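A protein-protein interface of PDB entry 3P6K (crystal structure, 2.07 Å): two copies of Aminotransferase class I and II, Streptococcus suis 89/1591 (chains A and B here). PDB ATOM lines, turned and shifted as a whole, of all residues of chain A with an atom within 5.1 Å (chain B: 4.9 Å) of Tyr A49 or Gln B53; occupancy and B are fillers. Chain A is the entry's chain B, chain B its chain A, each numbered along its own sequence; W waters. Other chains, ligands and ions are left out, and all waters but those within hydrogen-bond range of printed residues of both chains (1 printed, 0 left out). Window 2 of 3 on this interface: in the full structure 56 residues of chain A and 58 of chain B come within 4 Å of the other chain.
Water W1 lies within hydrogen-bond range of O of Thr B55 (2.6 Å), O of Leu B52 (2.7 Å) and N of Leu A34 (2.9 Å).
Tyr A49 touches just these residues of chain B: Tyr B49 (3.3 Å) and Gln B53 (2.7 Å). Gln B53 touches just these residues of chain A: Thr A33, Leu A34, Glu A35 and Tyr A49. Printed residues of chain A within 4 Å of Tyr B49: Tyr A49 (3.3 Å) and Gln A53 (2.9 Å). Printed residues of chain A within 4 Å of Thr B55: Thr A33 (3.6 Å). Of the printed residues of chain B, Thr A33 touches Gln B53, Gly B54 and Thr B55. Of the printed residues of chain A, Leu B52 touches Leu A34 (3.9 Å). Glu A46 touches none of the printed residues of chain B. The nearest residue of chain B that does not touch Tyr A49 is Leu B52 (4.3 Å). The nearest residue of chain A that does not touch Gln B53 is Pro A45 (4.1 Å). The nearest printed residue of chain A that does not touch Gly B54 is Glu A35 (5.0 Å).
Hydrophobic or aromatic side chains of chain A within 4 Å of the printed part of chain B: Leu A34 and Tyr A49. Of the 7 printed residues of chain B, 5 touch a printed residue of chain A. Along chain B the printed residues that touch a printed residue of chain A span positions 49 to 55.
Among the printed residues, merely in contact across the chains: Thr A33 with Gln B53 (3.5 Å), Thr A33 with Gly B54 (3.9 Å), Thr A33 with Thr B55 (3.6 Å), Leu A34 with Leu B52 (3.9 Å), Leu A34 with Gln B53 (3.5 Å) and Tyr A49 with Tyr B49 (3.3 Å).
Tyr B49 touches its own counterpart, Tyr A49. Tyr A49 touches Gln B53, and with the chains exchanged Gln A53 touches Tyr B49. 6 positions are printed for both chains. Of the 9 pairs that touch across the chains among the printed residues, 3 have their exchanged pair printed and touching as well.
The side-chain hydroxyl (OH) of Tyr B49 is in hydrogen-bond range of the side-chain amide oxygen (OE1) of Gln A53. The backbone NH (N) of Glu A35 is in hydrogen-bond range of the backbone carbonyl oxygen (O) of Gln B53, 3.0 Å away. The side-chain amide oxygen (OE1) of Gln B53 sits at hydrogen-bond distance from the side-chain hydroxyl (OH) of Tyr A49, at 2.7 Å.
The backbone carbonyl oxygen of Lys B51 lies within hydrogen-bond range of the side-chain hydroxyl of Thr B55.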
ATOM      1  N   THR A  33      -1.535  21.690 -18.909  1.00  0.00           N
ATOM      2  CA  THR A  33      -2.094  20.432 -19.378  1.00  0.00           C
ATOM      3  C   THR A  33      -2.280  19.658 -18.075  1.00  0.00           C
ATOM      4  O   THR A  33      -1.684  19.993 -17.033  1.00  0.00           O
ATOM      5  CB  THR A  33      -1.145  19.617 -20.292  1.00  0.00           C
ATOM      6  OG1 THR A  33       0.024  19.262 -19.537  1.00  0.00           O
ATOM      7  CG2 THR A  33      -0.769  20.403 -21.551  1.00  0.00           C
ATOM      8  N   LEU A  34      -3.091  18.616 -18.133  1.00  0.00           N
ATOM      9  CA  LEU A  34      -3.338  17.766 -16.958  1.00  0.00           C
ATOM     10  C   LEU A  34      -2.039  17.078 -16.557  1.00  0.00           C
ATOM     11  O   LEU A  34      -1.755  16.962 -15.354  1.00  0.00           O
ATOM     12  CB  LEU A  34      -4.470  16.764 -17.225  1.00  0.00           C
ATOM     13  CG  LEU A  34      -5.322  16.318 -16.048  1.00  0.00           C
ATOM     14  CD1 LEU A  34      -6.030  17.552 -15.405  1.00  0.00           C
ATOM     15  CD2 LEU A  34      -6.329  15.238 -16.517  1.00  0.00           C
ATOM     16  N   GLU A  35      -1.236  16.663 -17.541  1.00  0.00           N
ATOM     17  CA  GLU A  35       0.083  16.056 -17.292  1.00  0.00           C
ATOM     18  C   GLU A  35       0.994  17.003 -16.466  1.00  0.00           C
ATOM     19  O   GLU A  35       1.580  16.566 -15.461  1.00  0.00           O
ATOM     20  CB  GLU A  35       0.726  15.664 -18.640  1.00  0.00           C
ATOM     21  CG  GLU A  35       2.099  14.975 -18.633  1.00  0.00           C
ATOM     22  CD  GLU A  35       2.110  13.481 -18.396  1.00  0.00           C
ATOM     23  OE1 GLU A  35       1.065  12.757 -18.412  1.00  0.00           O
ATOM     24  OE2 GLU A  35       3.246  12.996 -18.216  1.00  0.00           O
ATOM     25  N   PHE A  38      -0.373  17.306 -12.875  1.00  0.00           N
ATOM     26  CA  PHE A  38       0.033  16.108 -12.126  1.00  0.00           C
ATOM     27  C   PHE A  38       1.515  16.172 -11.725  1.00  0.00           C
ATOM     28  O   PHE A  38       1.824  15.914 -10.572  1.00  0.00           O
ATOM     29  CB  PHE A  38      -0.189  14.805 -12.903  1.00  0.00           C
ATOM     30  CG  PHE A  38      -1.632  14.492 -13.242  1.00  0.00           C
ATOM     31  CD1 PHE A  38      -2.666  14.694 -12.331  1.00  0.00           C
ATOM     32  CD2 PHE A  38      -1.934  13.875 -14.455  1.00  0.00           C
ATOM     33  CE1 PHE A  38      -3.996  14.365 -12.664  1.00  0.00           C
ATOM     34  CE2 PHE A  38      -3.251  13.517 -14.780  1.00  0.00           C
ATOM     35  CZ  PHE A  38      -4.285  13.758 -13.868  1.00  0.00           C
ATOM     36  N   PRO A  45      -1.049   9.978 -11.919  1.00  0.00           N
ATOM     37  CA  PRO A  45      -2.179  10.073 -12.860  1.00  0.00           C
ATOM     38  C   PRO A  45      -3.259   8.985 -12.742  1.00  0.00           C
ATOM     39  O   PRO A  45      -4.452   9.306 -12.785  1.00  0.00           O
ATOM     40  CB  PRO A  45      -1.489  10.017 -14.238  1.00  0.00           C
ATOM     41  CG  PRO A  45      -0.160  10.636 -13.983  1.00  0.00           C
ATOM     42  CD  PRO A  45       0.239  10.090 -12.640  1.00  0.00           C
ATOM     43  N   GLU A  46      -2.844   7.735 -12.576  1.00  0.00           N
ATOM     44  CA  GLU A  46      -3.793   6.616 -12.425  1.00  0.00           C
ATOM     45  C   GLU A  46      -4.774   6.771 -11.255  1.00  0.00           C
ATOM     46  O   GLU A  46      -5.941   6.439 -11.391  1.00  0.00           O
ATOM     47  CB  GLU A  46      -3.082   5.236 -12.367  1.00  0.00           C
ATOM     48  CG  GLU A  46      -3.218   4.382 -13.663  1.00  0.00           C
ATOM     49  CD  GLU A  46      -2.507   4.930 -14.925  1.00  0.00           C
ATOM     50  OE1 GLU A  46      -2.701   6.101 -15.313  1.00  0.00           O
ATOM     51  OE2 GLU A  46      -1.775   4.127 -15.563  1.00  0.00           O
ATOM     52  N   ASP A  47      -4.292   7.260 -10.116  1.00  0.00           N
ATOM     53  CA  ASP A  47      -5.149   7.485  -8.945  1.00  0.00           C
ATOM     54  C   ASP A  47      -6.241   8.529  -9.266  1.00  0.00           C
ATOM     55  O   ASP A  47      -7.378   8.378  -8.832  1.00  0.00           O
ATOM     56  CB  ASP A  47      -4.354   7.991  -7.735  1.00  0.00           C
ATOM     57  CG  ASP A  47      -3.402   6.936  -7.127  1.00  0.00           C
ATOM     58  OD1 ASP A  47      -3.548   5.702  -7.322  1.00  0.00           O
ATOM     59  OD2 ASP A  47      -2.508   7.381  -6.390  1.00  0.00           O
ATOM     60  N   PHE A  48      -5.870   9.591  -9.980  1.00  0.00           N
ATOM     61  CA  PHE A  48      -6.819  10.618 -10.383  1.00  0.00           C
ATOM     62  C   PHE A  48      -7.857  10.050 -11.375  1.00  0.00           C
ATOM     63  O   PHE A  48      -9.044  10.323 -11.207  1.00  0.00           O
ATOM     64  CB  PHE A  48      -6.103  11.840 -10.976  1.00  0.00           C
ATOM     65  CG  PHE A  48      -7.019  12.938 -11.368  1.00  0.00           C
ATOM     66  CD1 PHE A  48      -7.580  12.975 -12.646  1.00  0.00           C
ATOM     67  CD2 PHE A  48      -7.327  13.957 -10.462  1.00  0.00           C
ATOM     68  CE1 PHE A  48      -8.467  14.010 -13.018  1.00  0.00           C
ATOM     69  CE2 PHE A  48      -8.191  14.971 -10.806  1.00  0.00           C
ATOM     70  CZ  PHE A  48      -8.752  15.019 -12.104  1.00  0.00           C
ATOM     71  N   TYR A  49      -7.410   9.283 -12.386  1.00  0.00           N
ATOM     72  CA  TYR A  49      -8.340   8.701 -13.383  1.00  0.00           C
ATOM     73  C   TYR A  49      -9.280   7.678 -12.766  1.00  0.00           C
ATOM     74  O   TYR A  49     -10.438   7.639 -13.133  1.00  0.00           O
ATOM     75  CB  TYR A  49      -7.637   8.090 -14.602  1.00  0.00           C
ATOM     76  CG  TYR A  49      -6.809   9.075 -15.369  1.00  0.00           C
ATOM     77  CD1 TYR A  49      -7.360  10.293 -15.812  1.00  0.00           C
ATOM     78  CD2 TYR A  49      -5.483   8.808 -15.681  1.00  0.00           C
ATOM     79  CE1 TYR A  49      -6.614  11.198 -16.508  1.00  0.00           C
ATOM     80  CE2 TYR A  49      -4.726   9.727 -16.389  1.00  0.00           C
ATOM     81  CZ  TYR A  49      -5.308  10.909 -16.798  1.00  0.00           C
ATOM     82  OH  TYR A  49      -4.594  11.818 -17.490  1.00  0.00           O
ATOM     83  N   LYS A  50      -8.786   6.866 -11.833  1.00  0.00           N
ATOM     84  CA  LYS A  50      -9.645   5.899 -11.124  1.00  0.00           C
ATOM     85  C   LYS A  50     -10.713   6.650 -10.308  1.00  0.00           C
ATOM     86  O   LYS A  50     -11.864   6.229 -10.314  1.00  0.00           O
ATOM     87  CB  LYS A  50      -8.844   4.902 -10.254  1.00  0.00           C
ATOM     88  N   LYS A  51     -10.348   7.756  -9.646  1.00  0.00           N
ATOM     89  CA  LYS A  51     -11.318   8.605  -8.930  1.00  0.00           C
ATOM     90  C   LYS A  51     -12.362   9.151  -9.947  1.00  0.00           C
ATOM     91  O   LYS A  51     -13.577   8.962  -9.763  1.00  0.00           O
ATOM     92  CB  LYS A  51     -10.632   9.777  -8.169  1.00  0.00           C
ATOM     93  CG  LYS A  51     -11.578  10.652  -7.281  1.00  0.00           C
ATOM     94  CD  LYS A  51     -10.899  11.853  -6.535  1.00  0.00           C
ATOM     95  CE  LYS A  51     -11.878  12.442  -5.490  1.00  0.00           C
ATOM     96  NZ  LYS A  51     -11.728  13.885  -4.980  1.00  0.00           N
ATOM     97  N   LEU A  52     -11.871   9.754 -11.030  1.00  0.00           N
ATOM     98  CA  LEU A  52     -12.714  10.412 -12.047  1.00  0.00           C
ATOM     99  C   LEU A  52     -13.737   9.483 -12.676  1.00  0.00           C
ATOM    100  O   LEU A  52     -14.936   9.759 -12.645  1.00  0.00           O
ATOM    101  CB  LEU A  52     -11.848  11.006 -13.178  1.00  0.00           C
ATOM    102  CG  LEU A  52     -12.537  11.637 -14.405  1.00  0.00           C
ATOM    103  CD1 LEU A  52     -13.517  12.765 -14.003  1.00  0.00           C
ATOM    104  CD2 LEU A  52     -11.492  12.119 -15.369  1.00  0.00           C
ATOM    105  N   GLN A  53     -13.243   8.363 -13.186  1.00  0.00           N
ATOM    106  CA  GLN A  53     -14.061   7.452 -13.972  1.00  0.00           C
ATOM    107  C   GLN A  53     -15.200   6.719 -13.253  1.00  0.00           C
ATOM    108  O   GLN A  53     -16.100   6.242 -13.921  1.00  0.00           O
ATOM    109  CB  GLN A  53     -13.196   6.496 -14.766  1.00  0.00           C
ATOM    110  CG  GLN A  53     -12.578   5.346 -14.027  1.00  0.00           C
ATOM    111  CD  GLN A  53     -11.691   4.533 -14.935  1.00  0.00           C
ATOM    112  OE1 GLN A  53     -11.361   4.951 -16.043  1.00  0.00           O
ATOM    113  NE2 GLN A  53     -11.319   3.352 -14.482  1.00  0.00           N
ATOM    114  N   GLY A  54     -15.119   6.592 -11.933  1.00  0.00           N
ATOM    115  CA  GLY A  54     -16.214   6.062 -11.133  1.00  0.00           C
ATOM    116  C   GLY A  54     -17.133   7.167 -10.600  1.00  0.00           C
ATOM    117  O   GLY A  54     -18.089   6.872  -9.899  1.00  0.00           O
ATOM    118  N   TYR B  49      -7.638   8.951 -22.092  1.00  0.00           N
ATOM    119  CA  TYR B  49      -6.725   9.602 -21.136  1.00  0.00           C
ATOM    120  C   TYR B  49      -5.427  10.101 -21.763  1.00  0.00           C
ATOM    121  O   TYR B  49      -4.926  11.142 -21.323  1.00  0.00           O
ATOM    122  CB  TYR B  49      -6.457   8.771 -19.863  1.00  0.00           C
ATOM    123  CG  TYR B  49      -7.714   8.446 -19.104  1.00  0.00           C
ATOM    124  CD1 TYR B  49      -8.638   9.448 -18.779  1.00  0.00           C
ATOM    125  CD2 TYR B  49      -7.989   7.136 -18.678  1.00  0.00           C
ATOM    126  CE1 TYR B  49      -9.808   9.165 -18.101  1.00  0.00           C
ATOM    127  CE2 TYR B  49      -9.174   6.838 -17.980  1.00  0.00           C
ATOM    128  CZ  TYR B  49     -10.073   7.870 -17.702  1.00  0.00           C
ATOM    129  OH  TYR B  49     -11.228   7.633 -17.034  1.00  0.00           O
ATOM    130  N   LYS B  50      -4.927   9.398 -22.791  1.00  0.00           N
ATOM    131  CA  LYS B  50      -3.730   9.819 -23.545  1.00  0.00           C
ATOM    132  C   LYS B  50      -3.952  11.143 -24.277  1.00  0.00           C
ATOM    133  O   LYS B  50      -3.085  11.995 -24.261  1.00  0.00           O
ATOM    134  CB  LYS B  50      -3.290   8.745 -24.568  1.00  0.00           C
ATOM    135  CG  LYS B  50      -1.946   9.034 -25.281  1.00  0.00           C
ATOM    136  CD  LYS B  50      -1.527   7.882 -26.230  1.00  0.00           C
ATOM    137  CE  LYS B  50      -0.261   8.231 -27.027  1.00  0.00           C
ATOM    138  NZ  LYS B  50       0.173   7.101 -27.919  1.00  0.00           N
ATOM    139  N   LYS B  51      -5.101  11.298 -24.925  1.00  0.00           N
ATOM    140  CA  LYS B  51      -5.425  12.520 -25.637  1.00  0.00           C
ATOM    141  C   LYS B  51      -5.643  13.669 -24.614  1.00  0.00           C
ATOM    142  O   LYS B  51      -5.074  14.752 -24.752  1.00  0.00           O
ATOM    143  CB  LYS B  51      -6.673  12.301 -26.513  1.00  0.00           C
ATOM    144  CG  LYS B  51      -7.045  13.482 -27.463  1.00  0.00           C
ATOM    145  CD  LYS B  51      -8.332  13.151 -28.246  1.00  0.00           C
ATOM    146  CE  LYS B  51      -8.846  14.318 -29.095  1.00  0.00           C
ATOM    147  NZ  LYS B  51     -10.249  14.070 -29.598  1.00  0.00           N
ATOM    148  N   LEU B  52      -6.449  13.391 -23.587  1.00  0.00           N
ATOM    149  CA  LEU B  52      -6.773  14.337 -22.530  1.00  0.00           C
ATOM    150  C   LEU B  52      -5.547  14.914 -21.842  1.00  0.00           C
ATOM    151  O   LEU B  52      -5.395  16.138 -21.787  1.00  0.00           O
ATOM    152  CB  LEU B  52      -7.648  13.688 -21.430  1.00  0.00           C
ATOM    153  CG  LEU B  52      -7.974  14.564 -20.200  1.00  0.00           C
ATOM    154  CD1 LEU B  52      -8.684  15.856 -20.668  1.00  0.00           C
ATOM    155  CD2 LEU B  52      -8.762  13.782 -19.143  1.00  0.00           C
ATOM    156  N   GLN B  53      -4.700  14.042 -21.299  1.00  0.00           N
ATOM    157  CA  GLN B  53      -3.581  14.511 -20.474  1.00  0.00           C
ATOM    158  C   GLN B  53      -2.553  15.421 -21.131  1.00  0.00           C
ATOM    159  O   GLN B  53      -1.938  16.203 -20.433  1.00  0.00           O
ATOM    160  CB  GLN B  53      -2.949  13.411 -19.656  1.00  0.00           C
ATOM    161  CG  GLN B  53      -2.116  12.376 -20.327  1.00  0.00           C
ATOM    162  CD  GLN B  53      -1.726  11.225 -19.348  1.00  0.00           C
ATOM    163  OE1 GLN B  53      -2.077  11.234 -18.149  1.00  0.00           O
ATOM    164  NE2 GLN B  53      -0.985  10.243 -19.871  1.00  0.00           N
ATOM    165  N   GLY B  54      -2.418  15.326 -22.451  1.00  0.00           N
ATOM    166  CA  GLY B  54      -1.569  16.223 -23.234  1.00  0.00           C
ATOM    167  C   GLY B  54      -2.305  17.410 -23.849  1.00  0.00           C
ATOM    168  O   GLY B  54      -1.680  18.188 -24.566  1.00  0.00           O
ATOM    169  N   THR B  55      -3.607  17.562 -23.580  1.00  0.00           N
ATOM    170  CA  THR B  55      -4.423  18.668 -24.105  1.00  0.00           C
ATOM    171  C   THR B  55      -4.312  19.893 -23.183  1.00  0.00           C
ATOM    172  O   THR B  55      -4.551  19.785 -21.972  1.00  0.00           O
ATOM    173  CB  THR B  55      -5.913  18.261 -24.239  1.00  0.00           C
ATOM    174  OG1 THR B  55      -5.997  17.176 -25.155  1.00  0.00           O
ATOM    175  CG2 THR B  55      -6.799  19.377 -24.778  1.00  0.00           C
HETATM  176  O   HOH W   1      -5.305  18.218 -19.996  1.00  0.00           O
